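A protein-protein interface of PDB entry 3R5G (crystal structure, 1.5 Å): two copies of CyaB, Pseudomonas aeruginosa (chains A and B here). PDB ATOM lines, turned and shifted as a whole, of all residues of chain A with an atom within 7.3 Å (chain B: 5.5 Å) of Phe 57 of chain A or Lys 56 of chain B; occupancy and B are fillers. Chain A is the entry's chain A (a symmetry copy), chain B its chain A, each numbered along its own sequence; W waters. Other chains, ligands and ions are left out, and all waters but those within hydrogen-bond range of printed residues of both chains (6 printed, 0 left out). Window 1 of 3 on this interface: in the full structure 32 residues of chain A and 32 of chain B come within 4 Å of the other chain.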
ATOM      1  N   LEU A  36     -18.161   7.002 -30.313  1.00  0.00           N
ATOM      2  CA  LEU A  36     -18.739   5.666 -29.967  1.00  0.00           C
ATOM      3  C   LEU A  36     -18.507   4.647 -31.097  1.00  0.00           C
ATOM      4  O   LEU A  36     -18.214   3.431 -30.848  1.00  0.00           O
ATOM      5  CB  LEU A  36     -20.239   5.781 -29.658  1.00  0.00           C
ATOM      6  CG  LEU A  36     -21.035   4.503 -29.365  1.00  0.00           C
ATOM      7  CD1 LEU A  36     -20.362   3.783 -28.134  1.00  0.00           C
ATOM      8  CD2 LEU A  36     -22.494   4.881 -28.997  1.00  0.00           C
ATOM      9  N   TYR A  39     -14.933   3.389 -31.301  1.00  0.00           N
ATOM     10  CA  TYR A  39     -14.750   2.461 -30.150  1.00  0.00           C
ATOM     11  C   TYR A  39     -15.373   1.116 -30.398  1.00  0.00           C
ATOM     12  O   TYR A  39     -14.732   0.092 -30.273  1.00  0.00           O
ATOM     13  CB  TYR A  39     -15.337   3.088 -28.888  1.00  0.00           C
ATOM     14  CG  TYR A  39     -15.339   2.093 -27.741  1.00  0.00           C
ATOM     15  CD1 TYR A  39     -14.146   1.781 -27.002  1.00  0.00           C
ATOM     16  CD2 TYR A  39     -16.533   1.454 -27.363  1.00  0.00           C
ATOM     17  CE1 TYR A  39     -14.149   0.794 -25.981  1.00  0.00           C
ATOM     18  CE2 TYR A  39     -16.559   0.504 -26.314  1.00  0.00           C
ATOM     19  CZ  TYR A  39     -15.345   0.164 -25.657  1.00  0.00           C
ATOM     20  OH  TYR A  39     -15.278  -0.754 -24.637  1.00  0.00           O
ATOM     21  N   LEU A  40     -16.659   1.088 -30.804  1.00  0.00           N
ATOM     22  CA  LEU A  40     -17.303  -0.179 -31.012  1.00  0.00           C
ATOM     23  C   LEU A  40     -16.656  -0.969 -32.179  1.00  0.00           C
ATOM     24  O   LEU A  40     -16.554  -2.168 -32.157  1.00  0.00           O
ATOM     25  CB  LEU A  40     -18.815   0.049 -31.253  1.00  0.00           C
ATOM     26  CG  LEU A  40     -19.577   0.537 -30.034  1.00  0.00           C
ATOM     27  CD1 LEU A  40     -21.035   0.916 -30.459  1.00  0.00           C
ATOM     28  CD2 LEU A  40     -19.589  -0.445 -28.822  1.00  0.00           C
ATOM     29  N   ASN A  41     -16.211  -0.254 -33.235  1.00  0.00           N
ATOM     30  CA  ASN A  41     -15.574  -0.929 -34.353  1.00  0.00           C
ATOM     31  C   ASN A  41     -14.217  -1.542 -33.900  1.00  0.00           C
ATOM     32  O   ASN A  41     -13.948  -2.672 -34.212  1.00  0.00           O
ATOM     33  CB  ASN A  41     -15.293   0.091 -35.477  1.00  0.00           C
ATOM     34  CG  ASN A  41     -15.115  -0.584 -36.799  1.00  0.00           C
ATOM     35  OD1 ASN A  41     -15.910  -1.420 -37.228  1.00  0.00           O
ATOM     36  ND2 ASN A  41     -13.964  -0.318 -37.410  1.00  0.00           N
ATOM     37  N   MET A  43     -13.389  -2.351 -30.795  1.00  0.00           N
ATOM     38  CA  MET A  43     -13.675  -3.526 -29.926  1.00  0.00           C
ATOM     39  C   MET A  43     -14.123  -4.741 -30.691  1.00  0.00           C
ATOM     40  O   MET A  43     -13.755  -5.867 -30.385  1.00  0.00           O
ATOM     41  CB  MET A  43     -14.721  -3.188 -28.864  1.00  0.00           C
ATOM     42  CG  MET A  43     -14.297  -2.167 -27.893  1.00  0.00           C
ATOM     43  SD  MET A  43     -12.786  -2.524 -26.990  1.00  0.00           S
ATOM     44  CE  MET A  43     -11.596  -1.458 -27.819  1.00  0.00           C
ATOM     45  N   SER A  44     -14.958  -4.554 -31.734  1.00  0.00           N
ATOM     46  CA  SER A  44     -15.354  -5.621 -32.577  1.00  0.00           C
ATOM     47  C   SER A  44     -14.163  -6.349 -33.250  1.00  0.00           C
ATOM     48  O   SER A  44     -14.141  -7.581 -33.287  1.00  0.00           O
ATOM     49  CB  SER A  44     -16.330  -5.045 -33.620  1.00  0.00           C
ATOM     50  OG  SER A  44     -16.578  -6.064 -34.542  1.00  0.00           O
ATOM     51  N   LYS A  45     -13.196  -5.595 -33.753  1.00  0.00           N
ATOM     52  CA  LYS A  45     -12.053  -6.199 -34.330  1.00  0.00           C
ATOM     53  C   LYS A  45     -11.250  -7.057 -33.328  1.00  0.00           C
ATOM     54  O   LYS A  45     -10.817  -8.118 -33.658  1.00  0.00           O
ATOM     55  CB  LYS A  45     -11.115  -5.108 -34.843  1.00  0.00           C
ATOM     56  CG  LYS A  45     -11.722  -4.345 -36.065  1.00  0.00           C
ATOM     57  CD  LYS A  45     -10.674  -3.503 -36.669  1.00  0.00           C
ATOM     58  CE  LYS A  45     -11.226  -3.007 -38.008  1.00  0.00           C
ATOM     59  NZ  LYS A  45     -10.892  -1.600 -38.371  1.00  0.00           N
ATOM     60  N   ALA A  47     -12.523  -8.563 -30.556  1.00  0.00           N
ATOM     61  CA  ALA A  47     -13.293  -9.752 -30.279  1.00  0.00           C
ATOM     62  C   ALA A  47     -13.177 -10.753 -31.422  1.00  0.00           C
ATOM     63  O   ALA A  47     -13.009 -11.928 -31.146  1.00  0.00           O
ATOM     64  CB  ALA A  47     -14.778  -9.393 -30.062  1.00  0.00           C
ATOM     65  N   ILE A  54     -19.660 -11.981 -30.996  1.00  0.00           N
ATOM     66  CA  ILE A  54     -20.210 -10.694 -30.614  1.00  0.00           C
ATOM     67  C   ILE A  54     -21.700 -10.797 -30.565  1.00  0.00           C
ATOM     68  O   ILE A  54     -22.366 -11.132 -31.594  1.00  0.00           O
ATOM     69  CB  ILE A  54     -19.732  -9.521 -31.499  1.00  0.00           C
ATOM     70  CG1 ILE A  54     -18.227  -9.527 -31.515  1.00  0.00           C
ATOM     71  CG2 ILE A  54     -20.309  -8.258 -30.958  1.00  0.00           C
ATOM     72  CD1 ILE A  54     -17.634  -8.664 -32.661  1.00  0.00           C
ATOM     73  N   ASP A  55     -22.257 -10.473 -29.409  1.00  0.00           N
ATOM     74  CA  ASP A  55     -23.691 -10.671 -29.271  1.00  0.00           C
ATOM     75  C   ASP A  55     -24.403  -9.441 -29.666  1.00  0.00           C
ATOM     76  O   ASP A  55     -25.265  -9.455 -30.568  1.00  0.00           O
ATOM     77  CB  ASP A  55     -24.106 -11.047 -27.863  1.00  0.00           C
ATOM     78  CG  ASP A  55     -25.603 -11.312 -27.778  1.00  0.00           C
ATOM     79  OD1 ASP A  55     -26.410 -10.442 -28.215  1.00  0.00           O
ATOM     80  OD2 ASP A  55     -25.949 -12.367 -27.235  1.00  0.00           O
ATOM     81  N   LYS A  56     -24.086  -8.355 -29.017  1.00  0.00           N
ATOM     82  CA  LYS A  56     -24.770  -7.099 -29.281  1.00  0.00           C
ATOM     83  C   LYS A  56     -24.012  -6.012 -28.570  1.00  0.00           C
ATOM     84  O   LYS A  56     -23.087  -6.267 -27.679  1.00  0.00           O
ATOM     85  CB  LYS A  56     -26.222  -7.092 -28.775  1.00  0.00           C
ATOM     86  CG  LYS A  56     -26.284  -7.207 -27.235  1.00  0.00           C
ATOM     87  CD  LYS A  56     -27.688  -7.130 -26.661  1.00  0.00           C
ATOM     88  CE  LYS A  56     -28.649  -8.059 -27.390  1.00  0.00           C
ATOM     89  NZ  LYS A  56     -28.533  -9.410 -26.830  1.00  0.00           N
ATOM     90  N   PHE A  57     -24.327  -4.818 -29.020  1.00  0.00           N
ATOM     91  CA  PHE A  57     -23.958  -3.630 -28.348  1.00  0.00           C
ATOM     92  C   PHE A  57     -25.231  -2.964 -27.828  1.00  0.00           C
ATOM     93  O   PHE A  57     -26.330  -2.949 -28.496  1.00  0.00           O
ATOM     94  CB  PHE A  57     -23.219  -2.634 -29.248  1.00  0.00           C
ATOM     95  CG  PHE A  57     -22.099  -3.225 -30.037  1.00  0.00           C
ATOM     96  CD1 PHE A  57     -22.060  -3.036 -31.405  1.00  0.00           C
ATOM     97  CD2 PHE A  57     -21.101  -3.988 -29.449  1.00  0.00           C
ATOM     98  CE1 PHE A  57     -21.001  -3.599 -32.152  1.00  0.00           C
ATOM     99  CE2 PHE A  57     -20.050  -4.510 -30.146  1.00  0.00           C
ATOM    100  CZ  PHE A  57     -19.983  -4.305 -31.556  1.00  0.00           C
ATOM    101  N   VAL A  58     -25.126  -2.421 -26.627  1.00  0.00           N
ATOM    102  CA  VAL A  58     -26.198  -1.617 -26.048  1.00  0.00           C
ATOM    103  C   VAL A  58     -25.577  -0.288 -25.677  1.00  0.00           C
ATOM    104  O   VAL A  58     -24.950  -0.165 -24.616  1.00  0.00           O
ATOM    105  CB  VAL A  58     -26.851  -2.285 -24.859  1.00  0.00           C
ATOM    106  CG1 VAL A  58     -28.013  -1.418 -24.354  1.00  0.00           C
ATOM    107  CG2 VAL A  58     -27.374  -3.693 -25.268  1.00  0.00           C
ATOM    108  N   GLY A  59     -25.714   0.725 -26.513  1.00  0.00           N
ATOM    109  CA  GLY A  59     -24.891   1.924 -26.394  1.00  0.00           C
ATOM    110  C   GLY A  59     -23.364   1.583 -26.383  1.00  0.00           C
ATOM    111  O   GLY A  59     -22.807   0.982 -27.331  1.00  0.00           O
ATOM    112  N   ASP A  60     -22.667   1.923 -25.287  1.00  0.00           N
ATOM    113  CA  ASP A  60     -21.229   1.607 -25.177  1.00  0.00           C
ATOM    114  C   ASP A  60     -21.009   0.258 -24.528  1.00  0.00           C
ATOM    115  O   ASP A  60     -19.857  -0.172 -24.469  1.00  0.00           O
ATOM    116  CB  ASP A  60     -20.522   2.649 -24.298  1.00  0.00           C
ATOM    117  CG  ASP A  60     -21.191   2.798 -22.910  1.00  0.00           C
ATOM    118  OD1 ASP A  60     -22.411   2.941 -22.822  1.00  0.00           O
ATOM    119  OD2 ASP A  60     -20.524   2.717 -21.855  1.00  0.00           O
ATOM    120  N   CYS A  61     -22.087  -0.386 -24.076  1.00  0.00           N
ATOM    121  CA  CYS A  61     -21.933  -1.725 -23.526  1.00  0.00           C
ATOM    122  C   CYS A  61     -21.717  -2.820 -24.580  1.00  0.00           C
ATOM    123  O   CYS A  61     -22.452  -2.839 -25.577  1.00  0.00           O
ATOM    124  CB  CYS A  61     -23.178  -2.068 -22.749  1.00  0.00           C
ATOM    125  SG  CYS A  61     -23.074  -3.735 -21.925  1.00  0.00           S
ATOM    126  N   VAL A  62     -20.678  -3.641 -24.443  1.00  0.00           N
ATOM    127  CA  VAL A  62     -20.368  -4.702 -25.376  1.00  0.00           C
ATOM    128  C   VAL A  62     -20.545  -6.065 -24.710  1.00  0.00           C
ATOM    129  O   VAL A  62     -20.123  -6.282 -23.577  1.00  0.00           O
ATOM    130  CB  VAL A  62     -18.912  -4.617 -25.754  1.00  0.00           C
ATOM    131  CG1 VAL A  62     -18.365  -5.794 -26.515  1.00  0.00           C
ATOM    132  CG2 VAL A  62     -18.601  -3.326 -26.548  1.00  0.00           C
ATOM    133  N   MET A  63     -21.209  -7.038 -25.327  1.00  0.00           N
ATOM    134  CA  MET A  63     -21.427  -8.367 -24.824  1.00  0.00           C
ATOM    135  C   MET A  63     -20.818  -9.341 -25.833  1.00  0.00           C
ATOM    136  O   MET A  63     -21.133  -9.224 -27.040  1.00  0.00           O
ATOM    137  CB  MET A  63     -22.926  -8.553 -24.761  1.00  0.00           C
ATOM    138  CG  MET A  63     -23.322  -9.816 -24.245  1.00  0.00           C
ATOM    139  SD  MET A  63     -25.177 -10.007 -24.344  1.00  0.00           S
ATOM    140  CE  MET A  63     -25.212 -11.735 -23.949  1.00  0.00           C
ATOM    141  N   VAL A  64     -19.940 -10.216 -25.396  1.00  0.00           N
ATOM    142  CA  VAL A  64     -19.244 -11.206 -26.238  1.00  0.00           C
ATOM    143  C   VAL A  64     -19.315 -12.516 -25.524  1.00  0.00           C
ATOM    144  O   VAL A  64     -19.251 -12.531 -24.263  1.00  0.00           O
ATOM    145  CB  VAL A  64     -17.791 -10.802 -26.485  1.00  0.00           C
ATOM    146  CG1 VAL A  64     -17.032 -11.865 -27.351  1.00  0.00           C
ATOM    147  CG2 VAL A  64     -17.719  -9.341 -27.040  1.00  0.00           C
ATOM    148  N   ARG A 129     -38.207  -9.656 -35.526  1.00  0.00           N
ATOM    149  CA  ARG A 129     -37.140  -9.081 -34.662  1.00  0.00           C
ATOM    150  C   ARG A 129     -36.520 -10.189 -33.800  1.00  0.00           C
ATOM    151  O   ARG A 129     -36.776 -10.307 -32.559  1.00  0.00           O
ATOM    152  CB  ARG A 129     -37.695  -7.992 -33.763  1.00  0.00           C
ATOM    153  CG  ARG A 129     -36.761  -6.816 -33.643  1.00  0.00           C
ATOM    154  CD  ARG A 129     -37.258  -5.657 -32.736  1.00  0.00           C
ATOM    155  NE  ARG A 129     -36.249  -4.587 -32.790  1.00  0.00           N
ATOM    156  CZ  ARG A 129     -36.421  -3.401 -33.363  1.00  0.00           C
ATOM    157  NH1 ARG A 129     -37.597  -3.053 -33.887  1.00  0.00           N
ATOM    158  NH2 ARG A 129     -35.422  -2.529 -33.358  1.00  0.00           N
ATOM    159  N   ASP A 131     -33.064 -12.639 -32.754  1.00  0.00           N
ATOM    160  CA  ASP A 131     -31.613 -12.672 -32.658  1.00  0.00           C
ATOM    161  C   ASP A 131     -31.075 -13.930 -32.010  1.00  0.00           C
ATOM    162  O   ASP A 131     -31.674 -14.551 -31.130  1.00  0.00           O
ATOM    163  CB  ASP A 131     -31.071 -11.432 -32.012  1.00  0.00           C
ATOM    164  CG  ASP A 131     -31.322 -10.201 -32.854  1.00  0.00           C
ATOM    165  OD1 ASP A 131     -30.557  -9.951 -33.855  1.00  0.00           O
ATOM    166  OD2 ASP A 131     -32.328  -9.516 -32.535  1.00  0.00           O
ATOM    167  N   ILE B  54     -39.693   0.118 -31.172  1.00  0.00           N
ATOM    168  CA  ILE B  54     -39.042  -0.985 -30.493  1.00  0.00           C
ATOM    169  C   ILE B  54     -37.572  -0.919 -30.755  1.00  0.00           C
ATOM    170  O   ILE B  54     -37.117  -0.967 -31.942  1.00  0.00           O
ATOM    171  CB  ILE B  54     -39.636  -2.370 -30.833  1.00  0.00           C
ATOM    172  CG1 ILE B  54     -41.117  -2.321 -30.573  1.00  0.00           C
ATOM    173  CG2 ILE B  54     -38.930  -3.398 -30.019  1.00  0.00           C
ATOM    174  CD1 ILE B  54     -41.884  -3.497 -31.236  1.00  0.00           C
ATOM    175  N   ASP B  55     -36.802  -0.857 -29.681  1.00  0.00           N
ATOM    176  CA  ASP B  55     -35.373  -0.670 -29.883  1.00  0.00           C
ATOM    177  C   ASP B  55     -34.707  -1.984 -29.971  1.00  0.00           C
ATOM    178  O   ASP B  55     -34.027  -2.298 -30.968  1.00  0.00           O
ATOM    179  CB  ASP B  55     -34.719   0.139 -28.782  1.00  0.00           C
ATOM    180  CG  ASP B  55     -33.241   0.370 -29.067  1.00  0.00           C
ATOM    181  OD1 ASP B  55     -32.501  -0.622 -29.330  1.00  0.00           O
ATOM    182  OD2 ASP B  55     -32.835   1.534 -28.980  1.00  0.00           O
ATOM    183  N   LYS B  56     -34.865  -2.782 -28.950  1.00  0.00           N
ATOM    184  CA  LYS B  56     -34.202  -4.075 -28.902  1.00  0.00           C
ATOM    185  C   LYS B  56     -34.781  -4.838 -27.743  1.00  0.00           C
ATOM    186  O   LYS B  56     -35.534  -4.272 -26.835  1.00  0.00           O
ATOM    187  CB  LYS B  56     -32.682  -3.959 -28.699  1.00  0.00           C
ATOM    188  CG  LYS B  56     -32.341  -3.341 -27.324  1.00  0.00           C
ATOM    189  CD  LYS B  56     -30.854  -3.267 -27.027  1.00  0.00           C
ATOM    190  CE  LYS B  56     -30.073  -2.664 -28.187  1.00  0.00           C
ATOM    191  NZ  LYS B  56     -30.127  -1.200 -28.096  1.00  0.00           N
ATOM    192  N   PHE B  57     -34.516  -6.124 -27.821  1.00  0.00           N
ATOM    193  CA  PHE B  57     -34.717  -7.008 -26.736  1.00  0.00           C
ATOM    194  C   PHE B  57     -33.350  -7.503 -26.268  1.00  0.00           C
ATOM    195  O   PHE B  57     -32.393  -7.775 -27.083  1.00  0.00           O
ATOM    196  CB  PHE B  57     -35.578  -8.223 -27.101  1.00  0.00           C
ATOM    197  CG  PHE B  57     -36.842  -7.893 -27.821  1.00  0.00           C
ATOM    198  CD1 PHE B  57     -37.126  -8.525 -29.017  1.00  0.00           C
ATOM    199  CD2 PHE B  57     -37.738  -6.946 -27.348  1.00  0.00           C
ATOM    200  CE1 PHE B  57     -38.321  -8.209 -29.700  1.00  0.00           C
ATOM    201  CE2 PHE B  57     -38.915  -6.653 -27.973  1.00  0.00           C
ATOM    202  CZ  PHE B  57     -39.234  -7.313 -29.196  1.00  0.00           C
ATOM    203  N   VAL B  58     -33.215  -7.612 -24.957  1.00  0.00           N
ATOM    204  CA  VAL B  58     -32.030  -8.211 -24.351  1.00  0.00           C
ATOM    205  C   VAL B  58     -32.530  -9.321 -23.451  1.00  0.00           C
ATOM    206  O   VAL B  58     -32.947  -9.064 -22.314  1.00  0.00           O
ATOM    207  CB  VAL B  58     -31.191  -7.206 -23.594  1.00  0.00           C
ATOM    208  CG1 VAL B  58     -29.928  -7.893 -23.051  1.00  0.00           C
ATOM    209  CG2 VAL B  58     -30.797  -6.033 -24.537  1.00  0.00           C
ATOM    210  N   CYS B  61     -35.666  -8.584 -21.361  1.00  0.00           N
ATOM    211  CA  CYS B  61     -35.759  -7.134 -21.270  1.00  0.00           C
ATOM    212  C   CYS B  61     -36.201  -6.446 -22.569  1.00  0.00           C
ATOM    213  O   CYS B  61     -35.662  -6.784 -23.633  1.00  0.00           O
ATOM    214  CB  CYS B  61     -34.404  -6.592 -20.895  1.00  0.00           C
ATOM    215  SG  CYS B  61     -34.407  -4.744 -20.667  1.00  0.00           S
ATOM    216  N   VAL B  62     -37.222  -5.594 -22.525  1.00  0.00           N
ATOM    217  CA  VAL B  62     -37.732  -4.894 -23.683  1.00  0.00           C
ATOM    218  C   VAL B  62     -37.479  -3.393 -23.553  1.00  0.00           C
ATOM    219  O   VAL B  62     -37.691  -2.799 -22.500  1.00  0.00           O
ATOM    220  CB  VAL B  62     -39.229  -5.054 -23.737  1.00  0.00           C
ATOM    221  CG1 VAL B  62     -39.944  -4.181 -24.732  1.00  0.00           C
ATOM    222  CG2 VAL B  62     -39.639  -6.526 -23.985  1.00  0.00           C
ATOM    223  N   MET B  63     -36.971  -2.703 -24.570  1.00  0.00           N
ATOM    224  CA  MET B  63     -36.707  -1.290 -24.587  1.00  0.00           C
ATOM    225  C   MET B  63     -37.521  -0.689 -25.732  1.00  0.00           C
ATOM    226  O   MET B  63     -37.430  -1.211 -26.868  1.00  0.00           O
ATOM    227  CB  MET B  63     -35.228  -1.142 -24.867  1.00  0.00           C
ATOM    228  CG  MET B  63     -34.785   0.208 -24.883  1.00  0.00           C
ATOM    229  SD  MET B  63     -32.986   0.296 -25.379  1.00  0.00           S
ATOM    230  CE  MET B  63     -32.934   2.055 -25.595  1.00  0.00           C
ATOM    231  N   GLY B 125     -22.699   1.694 -33.739  1.00  0.00           N
ATOM    232  CA  GLY B 125     -22.204   0.394 -33.856  1.00  0.00           C
ATOM    233  C   GLY B 125     -20.878   0.261 -34.625  1.00  0.00           C
ATOM    234  O   GLY B 125     -20.202   1.274 -34.851  1.00  0.00           O
ATOM    235  N   ALA B 126     -20.531  -0.993 -34.866  1.00  0.00           N
ATOM    236  CA  ALA B 126     -19.390  -1.382 -35.671  1.00  0.00           C
ATOM    237  C   ALA B 126     -19.859  -1.555 -37.119  1.00  0.00           C
ATOM    238  O   ALA B 126     -21.065  -1.648 -37.416  1.00  0.00           O
ATOM    239  CB  ALA B 126     -18.807  -2.656 -35.140  1.00  0.00           C
ATOM    240  N   ARG B 129     -22.231  -4.170 -38.001  1.00  0.00           N
ATOM    241  CA  ARG B 129     -23.102  -4.390 -36.814  1.00  0.00           C
ATOM    242  C   ARG B 129     -23.588  -3.040 -36.271  1.00  0.00           C
ATOM    243  O   ARG B 129     -23.112  -2.524 -35.210  1.00  0.00           O
ATOM    244  CB  ARG B 129     -22.357  -5.135 -35.722  1.00  0.00           C
ATOM    245  CG  ARG B 129     -23.215  -6.174 -35.049  1.00  0.00           C
ATOM    246  CD  ARG B 129     -22.523  -6.981 -33.915  1.00  0.00           C
ATOM    247  NE  ARG B 129     -23.490  -7.974 -33.424  1.00  0.00           N
ATOM    248  CZ  ARG B 129     -23.389  -9.288 -33.591  1.00  0.00           C
ATOM    249  NH1 ARG B 129     -22.319  -9.828 -34.175  1.00  0.00           N
ATOM    250  NH2 ARG B 129     -24.342 -10.077 -33.112  1.00  0.00           N
ATOM    251  N   THR B 133     -30.629   3.596 -32.609  1.00  0.00           N
ATOM    252  CA  THR B 133     -30.914   3.407 -31.149  1.00  0.00           C
ATOM    253  C   THR B 133     -30.643   4.716 -30.438  1.00  0.00           C
ATOM    254  O   THR B 133     -30.445   5.748 -31.070  1.00  0.00           O
ATOM    255  CB  THR B 133     -30.139   2.219 -30.606  1.00  0.00           C
ATOM    256  OG1 THR B 133     -30.426   1.967 -29.196  1.00  0.00           O
ATOM    257  CG2 THR B 133     -28.633   2.436 -30.829  1.00  0.00           C
HETATM  258  O   HOH W   1     -33.649  -7.271 -30.401  1.00  0.00           O
HETATM  259  O   HOH W   2     -27.293  -0.373 -29.534  1.00  0.00           O
HETATM  260  O   HOH W   3     -26.404  -7.298 -32.487  1.00  0.00           O
HETATM  261  O   HOH W   4     -28.719   0.752 -27.638  1.00  0.00           O
HETATM  262  O   HOH W   5     -31.556 -10.578 -27.362  1.00  0.00           O
HETATM  263  O   HOH W   6     -33.193  -5.006 -32.234  1.00  0.00           O
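The backbone carbonyl oxygen (O) of Asp 55 of chain A lies within hydrogen-bond range of the guanidinium group (NH2) of Arg 129 of chain B, 2.8 Å away. The backbone carbonyl oxygen of Ile 54 of chain A sits at hydrogen-bond distance from the guanidinium group of Arg 129 of chain B (2.7 Å). The backbone carbonyl oxygen (O) of Asp 55 of chain B lies within hydrogen-bond range of the guanidinium group (NH2) of Arg 129 of chain A (2.8 Å). O of Ile 54 of chain B is in hydrogen-bond range of NH2 of Arg 129 of chain A.
The backbone NH (N) of Met 63 of chain B is in hydrogen-bond range of the backbone carbonyl oxygen (O) of Lys 56 of chain B (3.1 Å). N of Asp 55 of chain A is in hydrogen-bond range of O of Met 63 of chain A (2.9 Å). OD1 of Asp 55 of chain B lies within salt-bridge range of NZ of Lys 56 of chain B (2.7 Å). OD2 of Asp 55 of chain B lies within hydrogen-bond range of OG1 of Thr 133 of chain B (2.5 Å). The backbone NH (N) of Met 63 of chain A lies within hydrogen-bond range of the backbone carbonyl oxygen (O) of Lys 56 of chain A (3.1 Å). The side-chain amide nitrogen (ND2) of Asn 41 of chain A sits close to the side-chain amino group (NZ) of Lys 45 of chain A (3.5 Å).
CA of Gly 125 of chain B touches CD1 of Leu 40 of chain A, 3.6 Å away. Leu 40 of chain A touches Ala 126 of chain B (O to CB, 3.8 Å). Ala 126 of chain B touches Ser 44 of chain A (CB to CB, 3.8 Å). Phe 57 of chain B touches Lys 56 of chain A (O to CE, 3.8 Å). CD of Lys 56 of chain A touches CG2 of Val 58 of chain B (3.9 Å). O of Phe 57 of chain A touches CE of Lys 56 of chain B, 3.8 Å away. Phe 57 of chain A touches Ala 126 of chain B (CE1 to N, 3.8 Å). Arg 129 of chain B touches Phe 57 of chain A. Val 58 of chain A touches Lys 56 of chain B. O of Arg 129 of chain A touches CE1 of Phe 57 of chain B, at 3.9 Å.
Phe 57 of chain A touches just these residues of chain B: Lys 56, Ala 126 and Arg 129. Of chain A, only Phe 57 (3.8 Å) and Val 58 (3.9 Å) come within 4 Å of Lys 56 of chain B. Of the printed residues of chain A, Ala 126 of chain B touches Leu 40 (3.8 Å), Asn 41 (3.7 Å), Ser 44 (3.8 Å) and Phe 57 (3.8 Å). Printed residues of chain B within 4 Å of Asn 41 of chain A: Ala 126 (3.7 Å). Printed residues of chain B within 4 Å of Arg 129 of chain A: Ile 54, Asp 55 and Phe 57. Of the printed residues of chain B, Asp 55 of chain A touches Arg 129. Of the printed residues of chain B, Lys 56 of chain A touches Phe 57 (3.8 Å) and Val 58 (3.9 Å). Asp 131 of chain A touches none of the printed residues of chain B. The nearest residue of chain B that does not touch Phe 57 of chain A is Gly 125 of chain B (4.2 Å). The nearest printed residue of chain A that does not touch Phe 57 of chain B is Asp 131 of chain A (5.7 Å).
Of the 12 printed residues of chain B, 8 touch a printed residue of chain A.
Ile 54 of chain A touches Arg 129 of chain B, and with the chains exchanged Arg 129 of chain A touches Ile 54 of chain B. Asp 55 of chain A touches Arg 129 of chain B, and with the chains exchanged Arg 129 of chain A touches Asp 55 of chain B. Lys 56 of chain A touches Phe 57 of chain B, and with the chains exchanged Phe 57 of chain A touches Lys 56 of chain B. Lys 56 of chain A touches Val 58 of chain B, and with the chains exchanged Val 58 of chain A touches Lys 56 of chain B.
Water W4 lies within hydrogen-bond range of the side-chain amino group of Lys 56 of chain B (2.5 Å), the side-chain hydroxyl of Thr 133 of chain B (2.6 Å) and the backbone NH of Gly 59 of chain A (3.2 Å). Water W2 bridges the backbone carbonyl oxygen of Phe 57 of chain A (2.9 Å) and the side-chain amino group of Lys 56 of chain B (3.3 Å). Water W5 lies within hydrogen-bond range of O of Phe 57 of chain B (2.9 Å) and NZ of Lys 56 of chain A (3.3 Å). Water W1 lies within hydrogen-bond range of the backbone NH (N) of Phe 57 of chain B and the side-chain carboxylate (OD2) of Asp 131 of chain A. Water W6 lies within hydrogen-bond range of O of Asp 55 of chain B (3.1 Å) and NE of Arg 129 of chain A (3.1 Å). Water W3 lies within hydrogen-bond range of the backbone carbonyl oxygen (O) of Asp 55 of chain A and the guanidinium group (NE) of Arg 129 of chain B.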
